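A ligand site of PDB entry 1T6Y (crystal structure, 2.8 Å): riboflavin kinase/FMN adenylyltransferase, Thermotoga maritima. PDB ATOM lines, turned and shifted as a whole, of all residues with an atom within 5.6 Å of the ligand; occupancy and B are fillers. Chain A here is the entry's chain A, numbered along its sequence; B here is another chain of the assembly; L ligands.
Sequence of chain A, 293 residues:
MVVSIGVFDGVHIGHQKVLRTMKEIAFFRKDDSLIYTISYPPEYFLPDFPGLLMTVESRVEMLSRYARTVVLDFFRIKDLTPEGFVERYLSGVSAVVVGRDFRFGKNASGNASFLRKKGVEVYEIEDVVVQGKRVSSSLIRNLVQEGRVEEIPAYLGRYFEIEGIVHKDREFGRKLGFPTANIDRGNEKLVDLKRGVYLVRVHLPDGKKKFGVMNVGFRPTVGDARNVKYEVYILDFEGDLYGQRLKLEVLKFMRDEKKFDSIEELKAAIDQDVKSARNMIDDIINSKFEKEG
Ile 5 touches the ligand.
Gly 6 touches the ligand.
Gly 14 touches the ligand.
CG2 of Val 18 touches O5 of the ligand, 3.6 Å away.
CA of Val 98 touches O6 of the ligand (3.6 Å).
Ile 125 touches the ligand.
O of Glu 126 touches C9 of the ligand, at 3.9 Å.
Asp 127 touches the ligand.
Hydrophobic or aromatic side chains within 4 Å of the ligand: Val 7, His 12, His 15, Val 18, Val 98, Val 128 and Val 135.
Within 4 Å of the ligand: Ile 5, Gly 6, Val 7, Phe 8, His 12, Gly 14, His 15, Val 18, Val 98, Gly 99, Asp 101, Ile 125, Glu 126, Asp 127, Val 128 and Val 135.
N of Val 135 is in hydrogen-bond range of O of Val 128, 3.1 Å away.
The backbone carbonyl oxygen (O) of Val 135 lies within hydrogen-bond range of a ring nitrogen (NE2) of His 12, at 3.5 Å.
ND1 of His 15 is in hydrogen-bond range of N of His 12, 2.8 Å away.
A ring nitrogen (NE2) of His 12 sits close to the backbone NH (N) of Ser 136 (3.4 Å).
The backbone carbonyl oxygen (O) of Val 98 lies within hydrogen-bond range of the backbone NH (N) of Ile 125 (2.8 Å).
An oxygen (O7) of the ligand is in hydrogen-bond range of the side-chain carboxylate of Asp 101 (2.5 Å).
The backbone NH of Val 128 is in hydrogen-bond range of a nitrogen (N4) of the ligand.
The backbone carbonyl oxygen of Val 128 is in hydrogen-bond range of a nitrogen (N3) of the ligand (3.3 Å).
A nitrogen (N3) of the ligand sits at hydrogen-bond distance from the backbone carbonyl oxygen (O) of Val 135, 2.7 Å away.
O3 of the ligand is in hydrogen-bond range of NE2 of His 15 (2.7 Å).
O7 of the ligand lies close to N of Gly 99 (3.0 Å).
The backbone NH (N) of Val 7 is in hydrogen-bond range of an oxygen (O1) of the ligand, at 2.9 Å.
N2 of the ligand lies within hydrogen-bond range of NE2 of His 12 (3.2 Å).
N of Phe 8 is in hydrogen-bond range of O3 of the ligand, at 3.3 Å.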
ATOM      1  N   ILE A   5      -6.247 -15.972  16.548  1.00  0.00           N
ATOM      2  CA  ILE A   5      -7.492 -15.894  17.287  1.00  0.00           C
ATOM      3  C   ILE A   5      -7.494 -14.646  18.192  1.00  0.00           C
ATOM      4  O   ILE A   5      -6.452 -14.024  18.368  1.00  0.00           O
ATOM      5  CB  ILE A   5      -7.653 -17.167  18.145  1.00  0.00           C
ATOM      6  CG1 ILE A   5      -7.274 -18.374  17.288  1.00  0.00           C
ATOM      7  CG2 ILE A   5      -9.078 -17.277  18.719  1.00  0.00           C
ATOM      8  CD1 ILE A   5      -7.323 -19.728  18.017  1.00  0.00           C
ATOM      9  N   GLY A   6      -8.653 -14.295  18.749  1.00  0.00           N
ATOM     10  CA  GLY A   6      -8.740 -13.154  19.655  1.00  0.00           C
ATOM     11  C   GLY A   6      -9.837 -12.146  19.370  1.00  0.00           C
ATOM     12  O   GLY A   6     -10.592 -12.274  18.394  1.00  0.00           O
ATOM     13  N   VAL A   7      -9.956 -11.136  20.225  1.00  0.00           N
ATOM     14  CA  VAL A   7     -10.962 -10.106  20.031  1.00  0.00           C
ATOM     15  C   VAL A   7     -10.504  -9.084  19.010  1.00  0.00           C
ATOM     16  O   VAL A   7     -11.233  -8.748  18.075  1.00  0.00           O
ATOM     17  CB  VAL A   7     -11.318  -9.378  21.351  1.00  0.00           C
ATOM     18  CG1 VAL A   7     -12.239  -8.160  21.045  1.00  0.00           C
ATOM     19  CG2 VAL A   7     -11.995 -10.343  22.308  1.00  0.00           C
ATOM     20  N   PHE A   8      -9.298  -8.561  19.176  1.00  0.00           N
ATOM     21  CA  PHE A   8      -8.770  -7.612  18.203  1.00  0.00           C
ATOM     22  C   PHE A   8      -9.512  -6.308  18.188  1.00  0.00           C
ATOM     23  O   PHE A   8      -9.454  -5.598  17.174  1.00  0.00           O
ATOM     24  CB  PHE A   8      -8.834  -8.189  16.785  1.00  0.00           C
ATOM     25  CG  PHE A   8      -7.990  -9.402  16.582  1.00  0.00           C
ATOM     26  CD1 PHE A   8      -6.639  -9.282  16.336  1.00  0.00           C
ATOM     27  CD2 PHE A   8      -8.559 -10.680  16.668  1.00  0.00           C
ATOM     28  CE1 PHE A   8      -5.845 -10.402  16.162  1.00  0.00           C
ATOM     29  CE2 PHE A   8      -7.784 -11.810  16.500  1.00  0.00           C
ATOM     30  CZ  PHE A   8      -6.419 -11.672  16.245  1.00  0.00           C
ATOM     31  N   ASP A   9     -10.195  -5.983  19.300  1.00  0.00           N
ATOM     32  CA  ASP A   9     -10.982  -4.750  19.401  1.00  0.00           C
ATOM     33  C   ASP A   9     -10.089  -3.571  19.262  1.00  0.00           C
ATOM     34  O   ASP A   9      -9.112  -3.436  19.990  1.00  0.00           O
ATOM     35  CB  ASP A   9     -11.702  -4.680  20.752  1.00  0.00           C
ATOM     36  CG  ASP A   9     -12.342  -3.288  21.035  1.00  0.00           C
ATOM     37  OD1 ASP A   9     -12.244  -2.907  22.199  1.00  0.00           O
ATOM     38  OD2 ASP A   9     -12.931  -2.611  20.148  1.00  0.00           O
ATOM     39  N   HIS A  12      -5.204  -2.626  17.508  1.00  0.00           N
ATOM     40  CA  HIS A  12      -4.050  -1.820  17.764  1.00  0.00           C
ATOM     41  C   HIS A  12      -2.755  -2.317  17.130  1.00  0.00           C
ATOM     42  O   HIS A  12      -2.718  -3.272  16.355  1.00  0.00           O
ATOM     43  CB  HIS A  12      -3.859  -1.585  19.256  1.00  0.00           C
ATOM     44  CG  HIS A  12      -3.795  -2.818  20.098  1.00  0.00           C
ATOM     45  ND1 HIS A  12      -4.914  -3.438  20.603  1.00  0.00           N
ATOM     46  CD2 HIS A  12      -2.738  -3.433  20.693  1.00  0.00           C
ATOM     47  CE1 HIS A  12      -4.568  -4.350  21.493  1.00  0.00           C
ATOM     48  NE2 HIS A  12      -3.249  -4.359  21.571  1.00  0.00           N
ATOM     49  N   GLY A  14      -0.252  -3.766  18.580  1.00  0.00           N
ATOM     50  CA  GLY A  14       0.185  -5.088  18.977  1.00  0.00           C
ATOM     51  C   GLY A  14      -0.620  -6.093  18.169  1.00  0.00           C
ATOM     52  O   GLY A  14      -0.233  -7.262  18.004  1.00  0.00           O
ATOM     53  N   HIS A  15      -1.751  -5.606  17.659  1.00  0.00           N
ATOM     54  CA  HIS A  15      -2.664  -6.400  16.860  1.00  0.00           C
ATOM     55  C   HIS A  15      -2.094  -6.578  15.457  1.00  0.00           C
ATOM     56  O   HIS A  15      -1.994  -7.690  14.937  1.00  0.00           O
ATOM     57  CB  HIS A  15      -4.039  -5.704  16.785  1.00  0.00           C
ATOM     58  CG  HIS A  15      -4.922  -5.948  17.977  1.00  0.00           C
ATOM     59  ND1 HIS A  15      -6.074  -5.215  18.218  1.00  0.00           N
ATOM     60  CD2 HIS A  15      -4.847  -6.866  18.979  1.00  0.00           C
ATOM     61  CE1 HIS A  15      -6.651  -5.674  19.319  1.00  0.00           C
ATOM     62  NE2 HIS A  15      -5.928  -6.673  19.796  1.00  0.00           N
ATOM     63  N   VAL A  18       0.828  -9.089  15.199  1.00  0.00           N
ATOM     64  CA  VAL A  18       0.281 -10.430  15.036  1.00  0.00           C
ATOM     65  C   VAL A  18      -0.282 -10.728  13.621  1.00  0.00           C
ATOM     66  O   VAL A  18       0.051 -11.732  12.989  1.00  0.00           O
ATOM     67  CB  VAL A  18      -0.841 -10.657  16.100  1.00  0.00           C
ATOM     68  CG1 VAL A  18      -1.559 -11.957  15.881  1.00  0.00           C
ATOM     69  CG2 VAL A  18      -0.208 -10.650  17.496  1.00  0.00           C
ATOM     70  N   VAL A  97      -1.524 -18.150  15.105  1.00  0.00           N
ATOM     71  CA  VAL A  97      -0.661 -17.050  15.465  1.00  0.00           C
ATOM     72  C   VAL A  97      -1.347 -16.333  16.642  1.00  0.00           C
ATOM     73  O   VAL A  97      -2.427 -15.755  16.485  1.00  0.00           O
ATOM     74  CB  VAL A  97      -0.509 -16.113  14.269  1.00  0.00           C
ATOM     75  CG1 VAL A  97       0.561 -15.079  14.539  1.00  0.00           C
ATOM     76  CG2 VAL A  97      -0.195 -16.935  13.005  1.00  0.00           C
ATOM     77  N   VAL A  98      -0.722 -16.388  17.811  1.00  0.00           N
ATOM     78  CA  VAL A  98      -1.262 -15.755  19.010  1.00  0.00           C
ATOM     79  C   VAL A  98      -0.209 -14.894  19.747  1.00  0.00           C
ATOM     80  O   VAL A  98       0.876 -14.646  19.225  1.00  0.00           O
ATOM     81  CB  VAL A  98      -1.813 -16.823  19.976  1.00  0.00           C
ATOM     82  CG1 VAL A  98      -3.012 -17.519  19.351  1.00  0.00           C
ATOM     83  CG2 VAL A  98      -0.734 -17.836  20.309  1.00  0.00           C
ATOM     84  N   GLY A  99      -0.544 -14.452  20.956  1.00  0.00           N
ATOM     85  CA  GLY A  99       0.383 -13.655  21.737  1.00  0.00           C
ATOM     86  C   GLY A  99       0.767 -14.399  23.006  1.00  0.00           C
ATOM     87  O   GLY A  99       0.199 -15.449  23.308  1.00  0.00           O
ATOM     88  N   ARG A 100       1.727 -13.859  23.760  1.00  0.00           N
ATOM     89  CA  ARG A 100       2.193 -14.499  24.995  1.00  0.00           C
ATOM     90  C   ARG A 100       1.102 -14.758  26.022  1.00  0.00           C
ATOM     91  O   ARG A 100       1.306 -15.511  26.973  1.00  0.00           O
ATOM     92  CB  ARG A 100       3.300 -13.667  25.638  1.00  0.00           C
ATOM     93  CG  ARG A 100       4.693 -13.911  25.087  1.00  0.00           C
ATOM     94  CD  ARG A 100       5.102 -15.381  25.233  1.00  0.00           C
ATOM     95  NE  ARG A 100       5.045 -15.851  26.611  1.00  0.00           N
ATOM     96  CZ  ARG A 100       5.099 -17.140  26.966  1.00  0.00           C
ATOM     97  NH1 ARG A 100       5.207 -18.084  26.042  1.00  0.00           N
ATOM     98  NH2 ARG A 100       5.052 -17.478  28.248  1.00  0.00           N
ATOM     99  N   ASP A 101      -0.054 -14.129  25.862  1.00  0.00           N
ATOM    100  CA  ASP A 101      -1.138 -14.290  26.809  1.00  0.00           C
ATOM    101  C   ASP A 101      -2.183 -15.317  26.395  1.00  0.00           C
ATOM    102  O   ASP A 101      -2.504 -16.230  27.153  1.00  0.00           O
ATOM    103  CB  ASP A 101      -1.806 -12.923  27.076  1.00  0.00           C
ATOM    104  CG  ASP A 101      -1.664 -11.960  25.894  1.00  0.00           C
ATOM    105  OD1 ASP A 101      -0.875 -10.988  25.972  1.00  0.00           O
ATOM    106  OD2 ASP A 101      -2.365 -12.168  24.887  1.00  0.00           O
ATOM    107  N   PHE A 102      -2.688 -15.189  25.179  1.00  0.00           N
ATOM    108  CA  PHE A 102      -3.717 -16.068  24.636  1.00  0.00           C
ATOM    109  C   PHE A 102      -4.085 -17.352  25.371  1.00  0.00           C
ATOM    110  O   PHE A 102      -3.287 -18.285  25.486  1.00  0.00           O
ATOM    111  CB  PHE A 102      -3.411 -16.423  23.196  1.00  0.00           C
ATOM    112  CG  PHE A 102      -4.508 -17.220  22.561  1.00  0.00           C
ATOM    113  CD1 PHE A 102      -5.721 -16.602  22.223  1.00  0.00           C
ATOM    114  CD2 PHE A 102      -4.379 -18.600  22.390  1.00  0.00           C
ATOM    115  CE1 PHE A 102      -6.788 -17.343  21.738  1.00  0.00           C
ATOM    116  CE2 PHE A 102      -5.450 -19.355  21.907  1.00  0.00           C
ATOM    117  CZ  PHE A 102      -6.658 -18.730  21.580  1.00  0.00           C
ATOM    118  N   ILE A 125       3.647 -14.581  19.154  1.00  0.00           N
ATOM    119  CA  ILE A 125       4.232 -13.266  18.916  1.00  0.00           C
ATOM    120  C   ILE A 125       4.452 -12.575  20.268  1.00  0.00           C
ATOM    121  O   ILE A 125       3.507 -12.247  20.978  1.00  0.00           O
ATOM    122  CB  ILE A 125       3.273 -12.390  18.059  1.00  0.00           C
ATOM    123  CG1 ILE A 125       3.320 -12.834  16.601  1.00  0.00           C
ATOM    124  CG2 ILE A 125       3.675 -10.924  18.170  1.00  0.00           C
ATOM    125  CD1 ILE A 125       4.686 -12.688  15.936  1.00  0.00           C
ATOM    126  N   GLU A 126       5.722 -12.375  20.623  1.00  0.00           N
ATOM    127  CA  GLU A 126       6.048 -11.720  21.901  1.00  0.00           C
ATOM    128  C   GLU A 126       5.511 -10.303  21.893  1.00  0.00           C
ATOM    129  O   GLU A 126       5.532  -9.625  20.862  1.00  0.00           O
ATOM    130  CB  GLU A 126       7.562 -11.719  22.152  1.00  0.00           C
ATOM    131  CG  GLU A 126       8.135 -13.109  22.382  1.00  0.00           C
ATOM    132  CD  GLU A 126       8.864 -13.226  23.695  1.00  0.00           C
ATOM    133  OE1 GLU A 126       9.421 -14.303  23.969  1.00  0.00           O
ATOM    134  OE2 GLU A 126       8.868 -12.236  24.456  1.00  0.00           O
ATOM    135  N   ASP A 127       5.054  -9.877  23.074  1.00  0.00           N
ATOM    136  CA  ASP A 127       4.421  -8.575  23.280  1.00  0.00           C
ATOM    137  C   ASP A 127       5.044  -7.291  22.782  1.00  0.00           C
ATOM    138  O   ASP A 127       6.222  -7.036  22.955  1.00  0.00           O
ATOM    139  CB  ASP A 127       4.029  -8.401  24.755  1.00  0.00           C
ATOM    140  CG  ASP A 127       4.741  -9.373  25.685  1.00  0.00           C
ATOM    141  OD1 ASP A 127       4.266  -9.527  26.839  1.00  0.00           O
ATOM    142  OD2 ASP A 127       5.753  -9.976  25.275  1.00  0.00           O
ATOM    143  N   VAL A 128       4.200  -6.491  22.139  1.00  0.00           N
ATOM    144  CA  VAL A 128       4.563  -5.188  21.613  1.00  0.00           C
ATOM    145  C   VAL A 128       4.389  -4.178  22.739  1.00  0.00           C
ATOM    146  O   VAL A 128       3.433  -4.291  23.505  1.00  0.00           O
ATOM    147  CB  VAL A 128       3.642  -4.765  20.488  1.00  0.00           C
ATOM    148  CG1 VAL A 128       4.072  -3.397  19.951  1.00  0.00           C
ATOM    149  CG2 VAL A 128       3.623  -5.818  19.411  1.00  0.00           C
ATOM    150  N   VAL A 129       5.273  -3.187  22.835  1.00  0.00           N
ATOM    151  CA  VAL A 129       5.130  -2.218  23.905  1.00  0.00           C
ATOM    152  C   VAL A 129       5.485  -0.820  23.497  1.00  0.00           C
ATOM    153  O   VAL A 129       6.606  -0.587  23.097  1.00  0.00           O
ATOM    154  CB  VAL A 129       5.969  -2.578  25.129  1.00  0.00           C
ATOM    155  CG1 VAL A 129       5.591  -3.968  25.623  1.00  0.00           C
ATOM    156  CG2 VAL A 129       7.439  -2.522  24.785  1.00  0.00           C
ATOM    157  N   ARG A 134       2.702  -2.748  27.583  1.00  0.00           N
ATOM    158  CA  ARG A 134       2.240  -3.699  26.571  1.00  0.00           C
ATOM    159  C   ARG A 134       0.974  -3.165  25.930  1.00  0.00           C
ATOM    160  O   ARG A 134      -0.058  -3.131  26.590  1.00  0.00           O
ATOM    161  CB  ARG A 134       1.882  -5.039  27.214  1.00  0.00           C
ATOM    162  CG  ARG A 134       2.801  -5.488  28.310  1.00  0.00           C
ATOM    163  CD  ARG A 134       2.246  -6.762  28.937  1.00  0.00           C
ATOM    164  NE  ARG A 134       2.909  -7.082  30.201  1.00  0.00           N
ATOM    165  CZ  ARG A 134       2.547  -8.085  30.994  1.00  0.00           C
ATOM    166  NH1 ARG A 134       1.539  -8.878  30.657  1.00  0.00           N
ATOM    167  NH2 ARG A 134       3.190  -8.292  32.133  1.00  0.00           N
ATOM    168  N   VAL A 135       1.033  -2.762  24.663  1.00  0.00           N
ATOM    169  CA  VAL A 135      -0.170  -2.256  24.006  1.00  0.00           C
ATOM    170  C   VAL A 135      -1.371  -3.178  24.281  1.00  0.00           C
ATOM    171  O   VAL A 135      -1.221  -4.402  24.421  1.00  0.00           O
ATOM    172  CB  VAL A 135       0.015  -2.155  22.483  1.00  0.00           C
ATOM    173  CG1 VAL A 135      -0.955  -1.140  21.918  1.00  0.00           C
ATOM    174  CG2 VAL A 135       1.437  -1.764  22.135  1.00  0.00           C
ATOM    175  N   SER A 136      -2.558  -2.599  24.389  1.00  0.00           N
ATOM    176  CA  SER A 136      -3.745  -3.391  24.677  1.00  0.00           C
ATOM    177  C   SER A 136      -4.949  -2.539  24.492  1.00  0.00           C
ATOM    178  O   SER A 136      -4.838  -1.318  24.506  1.00  0.00           O
ATOM    179  CB  SER A 136      -3.735  -3.862  26.099  1.00  0.00           C
ATOM    180  OG  SER A 136      -3.787  -2.725  26.911  1.00  0.00           O
ATOM    181  N   SER A 137      -6.105  -3.176  24.311  1.00  0.00           N
ATOM    182  CA  SER A 137      -7.355  -2.451  24.134  1.00  0.00           C
ATOM    183  C   SER A 137      -7.630  -1.691  25.433  1.00  0.00           C
ATOM    184  O   SER A 137      -8.091  -0.553  25.395  1.00  0.00           O
ATOM    185  CB  SER A 137      -8.494  -3.412  23.815  1.00  0.00           C
ATOM    186  OG  SER A 137      -8.387  -3.904  22.484  1.00  0.00           O
ATOM    187  N   LYS B 208      -5.078  -3.117  32.509  1.00  0.00           N
ATOM    188  CA  LYS B 208      -5.844  -4.355  32.424  1.00  0.00           C
ATOM    189  C   LYS B 208      -6.369  -4.755  33.800  1.00  0.00           C
ATOM    190  O   LYS B 208      -5.744  -4.466  34.819  1.00  0.00           O
ATOM    191  CB  LYS B 208      -4.952  -5.487  31.878  1.00  0.00           C
ATOM    192  CG  LYS B 208      -5.557  -6.311  30.730  1.00  0.00           C
ATOM    193  CD  LYS B 208      -5.421  -5.584  29.385  1.00  0.00           C
ATOM    194  CE  LYS B 208      -5.742  -6.470  28.184  1.00  0.00           C
ATOM    195  NZ  LYS B 208      -4.756  -7.566  27.975  1.00  0.00           N
HETATM  196  P1  LIG L   1      -6.975  -9.656  22.076  1.00  0.00           P
HETATM  197  O1  LIG L   1      -8.260 -10.289  22.387  1.00  0.00           O
HETATM  198  O2  LIG L   1      -5.964  -9.788  23.177  1.00  0.00           O
HETATM  199  O3  LIG L   1      -7.144  -8.219  21.621  1.00  0.00           O
HETATM  200  O4  LIG L   1      -6.431 -10.485  20.764  1.00  0.00           O
HETATM  201  C1  LIG L   1      -5.175 -10.015  20.323  1.00  0.00           C
HETATM  202  C2  LIG L   1      -4.263 -11.173  19.896  1.00  0.00           C
HETATM  203  O5  LIG L   1      -3.060 -10.399  19.660  1.00  0.00           O
HETATM  204  C3  LIG L   1      -4.000 -12.192  21.153  1.00  0.00           C
HETATM  205  O6  LIG L   1      -3.573 -13.455  20.451  1.00  0.00           O
HETATM  206  C4  LIG L   1      -2.818 -11.441  21.848  1.00  0.00           C
HETATM  207  O7  LIG L   1      -1.903 -12.279  22.468  1.00  0.00           O
HETATM  208  C5  LIG L   1      -2.073 -10.645  20.678  1.00  0.00           C
HETATM  209  N1  LIG L   1      -1.694  -9.335  21.218  1.00  0.00           N
HETATM  210  C6  LIG L   1      -2.529  -8.284  21.659  1.00  0.00           C
HETATM  211  N2  LIG L   1      -1.943  -7.177  22.115  1.00  0.00           N
HETATM  212  C7  LIG L   1      -0.613  -7.559  21.944  1.00  0.00           C
HETATM  213  C8  LIG L   1       0.574  -6.867  22.211  1.00  0.00           C
HETATM  214  N3  LIG L   1       0.488  -5.591  22.738  1.00  0.00           N
HETATM  215  N4  LIG L   1       1.760  -7.548  21.919  1.00  0.00           N
HETATM  216  C9  LIG L   1       1.796  -8.798  21.413  1.00  0.00           C
HETATM  217  N5  LIG L   1       0.705  -9.526  21.121  1.00  0.00           N
HETATM  218  C10 LIG L   1      -0.443  -8.861  21.408  1.00  0.00           C
